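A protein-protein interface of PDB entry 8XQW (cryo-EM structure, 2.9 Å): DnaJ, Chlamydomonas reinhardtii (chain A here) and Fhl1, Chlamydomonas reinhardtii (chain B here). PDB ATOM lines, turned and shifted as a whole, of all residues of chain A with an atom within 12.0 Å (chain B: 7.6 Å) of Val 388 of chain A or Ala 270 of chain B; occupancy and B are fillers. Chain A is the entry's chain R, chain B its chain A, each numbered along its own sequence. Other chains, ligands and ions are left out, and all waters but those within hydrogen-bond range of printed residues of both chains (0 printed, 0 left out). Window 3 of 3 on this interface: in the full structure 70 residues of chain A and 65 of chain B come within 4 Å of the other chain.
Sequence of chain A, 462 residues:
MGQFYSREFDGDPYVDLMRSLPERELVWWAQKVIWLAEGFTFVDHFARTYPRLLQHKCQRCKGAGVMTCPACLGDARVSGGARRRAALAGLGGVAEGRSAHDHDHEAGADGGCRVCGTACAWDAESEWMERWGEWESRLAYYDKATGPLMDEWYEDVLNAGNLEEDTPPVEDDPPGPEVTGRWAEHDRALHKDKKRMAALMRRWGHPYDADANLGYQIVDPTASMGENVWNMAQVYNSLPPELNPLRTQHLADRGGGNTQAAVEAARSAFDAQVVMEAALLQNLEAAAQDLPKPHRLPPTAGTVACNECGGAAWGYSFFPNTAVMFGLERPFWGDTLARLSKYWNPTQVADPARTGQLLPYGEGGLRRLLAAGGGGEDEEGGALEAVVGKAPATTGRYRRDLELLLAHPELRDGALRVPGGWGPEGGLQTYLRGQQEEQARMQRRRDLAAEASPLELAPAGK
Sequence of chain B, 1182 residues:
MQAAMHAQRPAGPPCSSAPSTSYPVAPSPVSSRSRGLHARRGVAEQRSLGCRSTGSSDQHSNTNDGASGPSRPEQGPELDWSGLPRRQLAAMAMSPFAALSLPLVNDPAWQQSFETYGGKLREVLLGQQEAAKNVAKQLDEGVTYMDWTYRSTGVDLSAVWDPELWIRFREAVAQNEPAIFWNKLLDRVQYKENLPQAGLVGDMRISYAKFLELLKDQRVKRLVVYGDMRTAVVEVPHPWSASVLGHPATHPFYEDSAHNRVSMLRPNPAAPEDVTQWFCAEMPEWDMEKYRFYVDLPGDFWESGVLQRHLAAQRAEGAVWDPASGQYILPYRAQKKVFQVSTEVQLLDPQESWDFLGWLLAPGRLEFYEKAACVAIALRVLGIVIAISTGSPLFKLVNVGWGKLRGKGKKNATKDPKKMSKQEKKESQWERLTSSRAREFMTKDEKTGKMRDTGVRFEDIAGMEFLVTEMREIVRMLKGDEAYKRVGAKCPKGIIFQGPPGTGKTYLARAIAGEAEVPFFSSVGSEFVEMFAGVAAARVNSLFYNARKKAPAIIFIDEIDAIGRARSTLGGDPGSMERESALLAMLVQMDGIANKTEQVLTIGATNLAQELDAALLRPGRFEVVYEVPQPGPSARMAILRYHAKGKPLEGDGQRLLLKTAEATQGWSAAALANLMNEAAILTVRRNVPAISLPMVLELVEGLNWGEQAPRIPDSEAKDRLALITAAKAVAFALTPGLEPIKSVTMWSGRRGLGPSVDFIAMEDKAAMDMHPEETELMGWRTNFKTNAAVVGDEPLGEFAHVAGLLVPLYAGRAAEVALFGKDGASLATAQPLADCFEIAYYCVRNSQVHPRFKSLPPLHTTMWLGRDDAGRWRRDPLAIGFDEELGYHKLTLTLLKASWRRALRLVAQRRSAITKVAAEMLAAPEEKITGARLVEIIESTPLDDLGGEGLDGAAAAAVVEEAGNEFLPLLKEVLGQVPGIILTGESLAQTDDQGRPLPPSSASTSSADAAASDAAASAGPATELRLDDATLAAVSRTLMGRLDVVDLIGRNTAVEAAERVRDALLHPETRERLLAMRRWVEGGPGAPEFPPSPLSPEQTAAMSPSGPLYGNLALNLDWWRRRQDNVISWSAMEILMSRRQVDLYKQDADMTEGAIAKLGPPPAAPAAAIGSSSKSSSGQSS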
ATOM      1  N   ALA A 383      24.105  28.242  -4.980  1.00  0.00           N
ATOM      2  CA  ALA A 383      23.824  29.667  -4.888  1.00  0.00           C
ATOM      3  C   ALA A 383      22.883  29.960  -3.727  1.00  0.00           C
ATOM      4  O   ALA A 383      23.287  29.963  -2.566  1.00  0.00           O
ATOM      5  CB  ALA A 383      23.232  30.174  -6.190  1.00  0.00           C
ATOM      6  N   LEU A 384      21.615  30.237  -4.069  1.00  0.00           N
ATOM      7  CA  LEU A 384      20.593  30.587  -3.050  1.00  0.00           C
ATOM      8  C   LEU A 384      19.767  29.350  -2.692  1.00  0.00           C
ATOM      9  O   LEU A 384      18.625  29.515  -2.249  1.00  0.00           O
ATOM     10  CB  LEU A 384      19.701  31.667  -3.651  1.00  0.00           C
ATOM     11  CG  LEU A 384      20.381  32.990  -4.010  1.00  0.00           C
ATOM     12  CD1 LEU A 384      20.256  33.242  -5.499  1.00  0.00           C
ATOM     13  CD2 LEU A 384      19.732  34.117  -3.232  1.00  0.00           C
ATOM     14  N   GLU A 385      20.348  28.167  -2.844  1.00  0.00           N
ATOM     15  CA  GLU A 385      19.633  26.916  -2.513  1.00  0.00           C
ATOM     16  C   GLU A 385      19.158  26.968  -1.058  1.00  0.00           C
ATOM     17  O   GLU A 385      18.154  26.317  -0.733  1.00  0.00           O
ATOM     18  CB  GLU A 385      20.587  25.751  -2.739  1.00  0.00           C
ATOM     19  CG  GLU A 385      19.960  24.386  -2.479  1.00  0.00           C
ATOM     20  CD  GLU A 385      20.349  23.353  -3.517  1.00  0.00           C
ATOM     21  OE1 GLU A 385      20.345  23.704  -4.714  1.00  0.00           O
ATOM     22  OE2 GLU A 385      20.652  22.205  -3.135  1.00  0.00           O
ATOM     23  N   ALA A 386      19.847  27.727  -0.215  1.00  0.00           N
ATOM     24  CA  ALA A 386      19.481  27.759   1.215  1.00  0.00           C
ATOM     25  C   ALA A 386      18.234  28.610   1.425  1.00  0.00           C
ATOM     26  O   ALA A 386      17.619  28.505   2.499  1.00  0.00           O
ATOM     27  CB  ALA A 386      20.626  28.307   2.011  1.00  0.00           C
ATOM     28  N   VAL A 387      17.885  29.445   0.451  1.00  0.00           N
ATOM     29  CA  VAL A 387      16.735  30.367   0.664  1.00  0.00           C
ATOM     30  C   VAL A 387      15.491  29.766   0.008  1.00  0.00           C
ATOM     31  O   VAL A 387      14.416  29.854   0.622  1.00  0.00           O
ATOM     32  CB  VAL A 387      17.027  31.769   0.105  1.00  0.00           C
ATOM     33  CG1 VAL A 387      16.140  32.831   0.738  1.00  0.00           C
ATOM     34  CG2 VAL A 387      18.497  32.139   0.251  1.00  0.00           C
ATOM     35  N   VAL A 388      15.642  29.153  -1.162  1.00  0.00           N
ATOM     36  CA  VAL A 388      14.450  28.672  -1.909  1.00  0.00           C
ATOM     37  C   VAL A 388      14.557  27.176  -2.192  1.00  0.00           C
ATOM     38  O   VAL A 388      14.009  26.743  -3.213  1.00  0.00           O
ATOM     39  CB  VAL A 388      14.411  29.463  -3.217  1.00  0.00           C
ATOM     40  CG1 VAL A 388      13.917  30.886  -2.994  1.00  0.00           C
ATOM     41  CG2 VAL A 388      15.766  29.451  -3.909  1.00  0.00           C
ATOM     42  N   GLY A 389      15.238  26.423  -1.338  1.00  0.00           N
ATOM     43  CA  GLY A 389      15.292  24.959  -1.507  1.00  0.00           C
ATOM     44  C   GLY A 389      16.081  24.540  -2.727  1.00  0.00           C
ATOM     45  O   GLY A 389      16.648  25.416  -3.406  1.00  0.00           O
ATOM     46  N   LYS A 390      16.133  23.234  -2.997  1.00  0.00           N
ATOM     47  CA  LYS A 390      16.892  22.710  -4.156  1.00  0.00           C
ATOM     48  C   LYS A 390      15.972  22.641  -5.366  1.00  0.00           C
ATOM     49  O   LYS A 390      14.741  22.657  -5.169  1.00  0.00           O
ATOM     50  CB  LYS A 390      17.326  21.276  -3.871  1.00  0.00           C
ATOM     51  CG  LYS A 390      16.313  20.453  -3.095  1.00  0.00           C
ATOM     52  CD  LYS A 390      16.970  19.366  -2.255  1.00  0.00           C
ATOM     53  CE  LYS A 390      18.370  19.723  -1.876  1.00  0.00           C
ATOM     54  NZ  LYS A 390      19.318  18.669  -2.242  1.00  0.00           N
ATOM     55  N   ALA A 391      16.534  22.558  -6.573  1.00  0.00           N
ATOM     56  CA  ALA A 391      15.611  22.401  -7.682  1.00  0.00           C
ATOM     57  C   ALA A 391      15.307  20.924  -7.904  1.00  0.00           C
ATOM     58  O   ALA A 391      16.224  20.099  -7.934  1.00  0.00           O
ATOM     59  CB  ALA A 391      16.192  23.006  -8.953  1.00  0.00           C
ATOM     60  N   PRO A 392      14.035  20.561  -8.057  1.00  0.00           N
ATOM     61  CA  PRO A 392      13.689  19.153  -8.278  1.00  0.00           C
ATOM     62  C   PRO A 392      14.048  18.741  -9.694  1.00  0.00           C
ATOM     63  O   PRO A 392      13.587  19.347 -10.662  1.00  0.00           O
ATOM     64  CB  PRO A 392      12.176  19.122  -8.053  1.00  0.00           C
ATOM     65  CG  PRO A 392      11.729  20.495  -8.399  1.00  0.00           C
ATOM     66  CD  PRO A 392      12.850  21.432  -8.057  1.00  0.00           C
ATOM     67  N   ALA A 393      14.878  17.714  -9.819  1.00  0.00           N
ATOM     68  CA  ALA A 393      15.227  17.191 -11.127  1.00  0.00           C
ATOM     69  C   ALA A 393      14.585  15.820 -11.294  1.00  0.00           C
ATOM     70  O   ALA A 393      15.225  14.776 -11.186  1.00  0.00           O
ATOM     71  CB  ALA A 393      16.743  17.124 -11.290  1.00  0.00           C
ATOM     72  N   PRO B 267       5.935  33.285  -8.637  1.00  0.00           N
ATOM     73  CA  PRO B 267       7.060  33.358  -9.580  1.00  0.00           C
ATOM     74  C   PRO B 267       8.444  33.018  -9.038  1.00  0.00           C
ATOM     75  O   PRO B 267       9.400  33.106  -9.813  1.00  0.00           O
ATOM     76  CB  PRO B 267       7.016  34.827 -10.023  1.00  0.00           C
ATOM     77  CG  PRO B 267       5.671  35.331  -9.602  1.00  0.00           C
ATOM     78  CD  PRO B 267       5.386  34.613  -8.351  1.00  0.00           C
ATOM     79  N   ASN B 268       8.600  32.621  -7.773  1.00  0.00           N
ATOM     80  CA  ASN B 268       9.903  32.179  -7.274  1.00  0.00           C
ATOM     81  C   ASN B 268      11.001  33.201  -7.541  1.00  0.00           C
ATOM     82  O   ASN B 268      11.785  33.028  -8.479  1.00  0.00           O
ATOM     83  CB  ASN B 268      10.303  30.839  -7.890  1.00  0.00           C
ATOM     84  CG  ASN B 268      11.522  30.225  -7.217  1.00  0.00           C
ATOM     85  OD1 ASN B 268      12.516  30.899  -6.954  1.00  0.00           O
ATOM     86  ND2 ASN B 268      11.443  28.939  -6.928  1.00  0.00           N
ATOM     87  N   PRO B 269      11.084  34.269  -6.754  1.00  0.00           N
ATOM     88  CA  PRO B 269      11.998  35.370  -7.093  1.00  0.00           C
ATOM     89  C   PRO B 269      13.447  34.960  -7.267  1.00  0.00           C
ATOM     90  O   PRO B 269      14.184  35.629  -8.001  1.00  0.00           O
ATOM     91  CB  PRO B 269      11.833  36.315  -5.900  1.00  0.00           C
ATOM     92  CG  PRO B 269      11.502  35.407  -4.780  1.00  0.00           C
ATOM     93  CD  PRO B 269      10.599  34.370  -5.371  1.00  0.00           C
ATOM     94  N   ALA B 270      13.886  33.882  -6.623  1.00  0.00           N
ATOM     95  CA  ALA B 270      15.305  33.549  -6.650  1.00  0.00           C
ATOM     96  C   ALA B 270      15.730  32.980  -7.994  1.00  0.00           C
ATOM     97  O   ALA B 270      16.896  33.107  -8.380  1.00  0.00           O
ATOM     98  CB  ALA B 270      15.636  32.561  -5.534  1.00  0.00           C
ATOM     99  N   ALA B 271      14.814  32.343  -8.719  1.00  0.00           N
ATOM    100  CA  ALA B 271      15.134  31.686  -9.983  1.00  0.00           C
ATOM    101  C   ALA B 271      13.998  31.894 -10.976  1.00  0.00           C
ATOM    102  O   ALA B 271      13.174  30.993 -11.187  1.00  0.00           O
ATOM    103  CB  ALA B 271      15.402  30.198  -9.776  1.00  0.00           C
ATOM    104  N   PRO B 272      13.927  33.057 -11.610  1.00  0.00           N
ATOM    105  CA  PRO B 272      13.014  33.208 -12.746  1.00  0.00           C
ATOM    106  C   PRO B 272      13.584  32.524 -13.976  1.00  0.00           C
ATOM    107  O   PRO B 272      14.618  31.855 -13.883  1.00  0.00           O
ATOM    108  CB  PRO B 272      12.921  34.726 -12.923  1.00  0.00           C
ATOM    109  CG  PRO B 272      14.216  35.227 -12.412  1.00  0.00           C
ATOM    110  CD  PRO B 272      14.627  34.312 -11.293  1.00  0.00           C
ATOM    111  N   GLN B 277      10.479  25.624 -11.426  1.00  0.00           N
ATOM    112  CA  GLN B 277      10.957  25.920 -10.088  1.00  0.00           C
ATOM    113  C   GLN B 277      10.099  26.951  -9.385  1.00  0.00           C
ATOM    114  O   GLN B 277      10.572  27.605  -8.456  1.00  0.00           O
ATOM    115  CB  GLN B 277      12.401  26.395 -10.142  1.00  0.00           C
ATOM    116  CG  GLN B 277      13.332  25.372 -10.729  1.00  0.00           C
ATOM    117  CD  GLN B 277      14.749  25.860 -10.769  1.00  0.00           C
ATOM    118  OE1 GLN B 277      15.148  26.702  -9.969  1.00  0.00           O
ATOM    119  NE2 GLN B 277      15.524  25.339 -11.707  1.00  0.00           N
ATOM    120  N   PHE B 279       6.502  28.133  -7.241  1.00  0.00           N
ATOM    121  CA  PHE B 279       5.736  27.595  -6.128  1.00  0.00           C
ATOM    122  C   PHE B 279       4.268  27.508  -6.501  1.00  0.00           C
ATOM    123  O   PHE B 279       3.762  28.339  -7.257  1.00  0.00           O
ATOM    124  CB  PHE B 279       5.906  28.455  -4.882  1.00  0.00           C
ATOM    125  CG  PHE B 279       7.325  28.640  -4.475  1.00  0.00           C
ATOM    126  CD1 PHE B 279       8.078  27.567  -4.065  1.00  0.00           C
ATOM    127  CD2 PHE B 279       7.908  29.882  -4.513  1.00  0.00           C
ATOM    128  CE1 PHE B 279       9.385  27.730  -3.697  1.00  0.00           C
ATOM    129  CE2 PHE B 279       9.212  30.048  -4.145  1.00  0.00           C
ATOM    130  CZ  PHE B 279       9.952  28.971  -3.738  1.00  0.00           C
ATOM    131  N   PRO B 331       8.797  30.096   5.619  1.00  0.00           N
ATOM    132  CA  PRO B 331       9.961  30.217   4.741  1.00  0.00           C
ATOM    133  C   PRO B 331       9.764  29.490   3.423  1.00  0.00           C
ATOM    134  O   PRO B 331       8.958  28.569   3.302  1.00  0.00           O
ATOM    135  CB  PRO B 331      11.087  29.588   5.562  1.00  0.00           C
ATOM    136  CG  PRO B 331      10.403  28.722   6.535  1.00  0.00           C
ATOM    137  CD  PRO B 331       9.123  29.395   6.866  1.00  0.00           C
ATOM    138  N   TYR B 332      10.522  29.930   2.419  1.00  0.00           N
ATOM    139  CA  TYR B 332      10.378  29.369   1.083  1.00  0.00           C
ATOM    140  C   TYR B 332      10.786  27.907   1.050  1.00  0.00           C
ATOM    141  O   TYR B 332      10.168  27.104   0.346  1.00  0.00           O
ATOM    142  CB  TYR B 332      11.207  30.169   0.089  1.00  0.00           C
ATOM    143  CG  TYR B 332      10.526  31.405  -0.424  1.00  0.00           C
ATOM    144  CD1 TYR B 332       9.165  31.424  -0.649  1.00  0.00           C
ATOM    145  CD2 TYR B 332      11.245  32.556  -0.683  1.00  0.00           C
ATOM    146  CE1 TYR B 332       8.539  32.553  -1.121  1.00  0.00           C
ATOM    147  CE2 TYR B 332      10.629  33.687  -1.151  1.00  0.00           C
ATOM    148  CZ  TYR B 332       9.277  33.682  -1.368  1.00  0.00           C
ATOM    149  OH  TYR B 332       8.661  34.814  -1.838  1.00  0.00           O
ATOM    150  N   ARG B 333      11.806  27.538   1.802  1.00  0.00           N
ATOM    151  CA  ARG B 333      12.256  26.156   1.726  1.00  0.00           C
ATOM    152  C   ARG B 333      11.334  25.206   2.416  1.00  0.00           C
ATOM    153  O   ARG B 333      11.671  24.031   2.567  1.00  0.00           O
ATOM    154  CB  ARG B 333      13.667  26.031   2.294  1.00  0.00           C
ATOM    155  CG  ARG B 333      13.738  25.986   3.794  1.00  0.00           C
ATOM    156  CD  ARG B 333      15.172  26.130   4.265  1.00  0.00           C
ATOM    157  NE  ARG B 333      15.532  27.531   4.445  1.00  0.00           N
ATOM    158  CZ  ARG B 333      15.235  28.240   5.526  1.00  0.00           C
ATOM    159  NH1 ARG B 333      14.572  27.679   6.526  1.00  0.00           N
ATOM    160  NH2 ARG B 333      15.598  29.512   5.606  1.00  0.00           N
ATOM    161  N   ALA B 334      10.162  25.670   2.838  1.00  0.00           N
ATOM    162  CA  ALA B 334       9.135  24.813   3.405  1.00  0.00           C
ATOM    163  C   ALA B 334       7.870  24.798   2.564  1.00  0.00           C
ATOM    164  O   ALA B 334       6.848  24.269   3.014  1.00  0.00           O
ATOM    165  CB  ALA B 334       8.803  25.245   4.832  1.00  0.00           C
ATOM    166  N   GLN B 335       7.903  25.367   1.366  1.00  0.00           N
ATOM    167  CA  GLN B 335       6.752  25.390   0.478  1.00  0.00           C
ATOM    168  C   GLN B 335       6.958  24.426  -0.679  1.00  0.00           C
ATOM    169  O   GLN B 335       8.084  24.072  -1.032  1.00  0.00           O
ATOM    170  CB  GLN B 335       6.499  26.799  -0.058  1.00  0.00           C
ATOM    171  CG  GLN B 335       5.512  27.586   0.766  1.00  0.00           C
ATOM    172  CD  GLN B 335       5.667  29.071   0.583  1.00  0.00           C
ATOM    173  OE1 GLN B 335       4.699  29.820   0.670  1.00  0.00           O
ATOM    174  NE2 GLN B 335       6.887  29.509   0.332  1.00  0.00           N
ATOM    175  N   LYS B 337       7.002  23.190  -4.453  1.00  0.00           N
ATOM    176  CA  LYS B 337       7.211  23.685  -5.803  1.00  0.00           C
ATOM    177  C   LYS B 337       6.175  23.048  -6.720  1.00  0.00           C
ATOM    178  O   LYS B 337       5.220  22.415  -6.268  1.00  0.00           O
ATOM    179  CB  LYS B 337       8.634  23.401  -6.258  1.00  0.00           C
ATOM    180  CG  LYS B 337       9.663  24.280  -5.609  1.00  0.00           C
ATOM    181  CD  LYS B 337      11.043  23.930  -6.096  1.00  0.00           C
ATOM    182  CE  LYS B 337      12.058  24.871  -5.513  1.00  0.00           C
ATOM    183  NZ  LYS B 337      11.754  25.104  -4.087  1.00  0.00           N
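Of the printed residues of chain B, Ala 386 of chain A touches Arg 333.
Of the printed residues of chain B, Val 387 of chain A touches Tyr 332 (3.3 Å) and Arg 333 (3.7 Å).
Val 388 of chain A touches three residues of chain B.
Gly 389 of chain A touches one residue of chain B.
No residue of chain A comes within 4 Å of Asn 268 of chain B.
No residue of chain A comes within 4 Å of Pro 269 of chain B.
Of chain A, only Val 388 comes within 4 Å of Ala 270 of chain B.
No residue of chain A comes within 4 Å of Ala 271 of chain B.
Pro 272 of chain B touches none of the printed residues of chain A.
Tyr 332 of chain B touches just these residues of chain A: Val 387 and Val 388.
The nearest residue of chain B that does not touch Val 388 of chain A is Asn 268 of chain B (4.2 Å).
The side-chain carboxylate (OE2) of Glu 385 of chain A is in salt-bridge range of the side-chain amino group (NZ) of Lys 390 of chain A (3.9 Å).
OD1 of Asn 268 of chain B lies close to N of Ala 270 of chain B (3.3 Å).
Printed residues of chain A that touch a printed residue of chain B: Ala 386, Val 387, Val 388, Gly 389, Lys 390, Ala 391 and Pro 392.
Hydrophobic or aromatic side chains of chain A that line the printed part of chain B: Val 388, Ala 391 and Pro 392.
Of the 14 printed residues of chain B, 5 touch a printed residue of chain A.
Along chain B the printed residues that touch a printed residue of chain A span positions 270 to 337.
Among the printed residues, 10 pairs touch across the chains.
Among the printed residues, no Asp or Glu carboxylate lies within 4 Å of a Lys or Arg side-chain nitrogen of the other chain.
CB of Tyr 332 of chain B touches O of Val 387 of chain A (3.3 Å).
Val 387 of chain A touches Arg 333 of chain B.
Val 388 of chain A touches Ala 270 of chain B (CG1 to CB, 3.5 Å).
Val 388 of chain A touches Tyr 332 of chain B.
Arg 333 of chain B touches Gly 389 of chain A (CB to N, 3.98 Å).
Lys 390 of chain A touches Lys 337 of chain B.
Ala 391 of chain A touches Gln 277 of chain B.
CD of Pro 392 of chain A touches CD of Lys 337 of chain B, at 3.7 Å.
The backbone carbonyl oxygen of Ala 386 of chain A is in hydrogen-bond range of the guanidinium group of Arg 333 of chain B (3.0 Å).
The side-chain amino group (NZ) of Lys 337 of chain B lies within hydrogen-bond range of the backbone carbonyl oxygen (O) of Val 388 of chain A.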
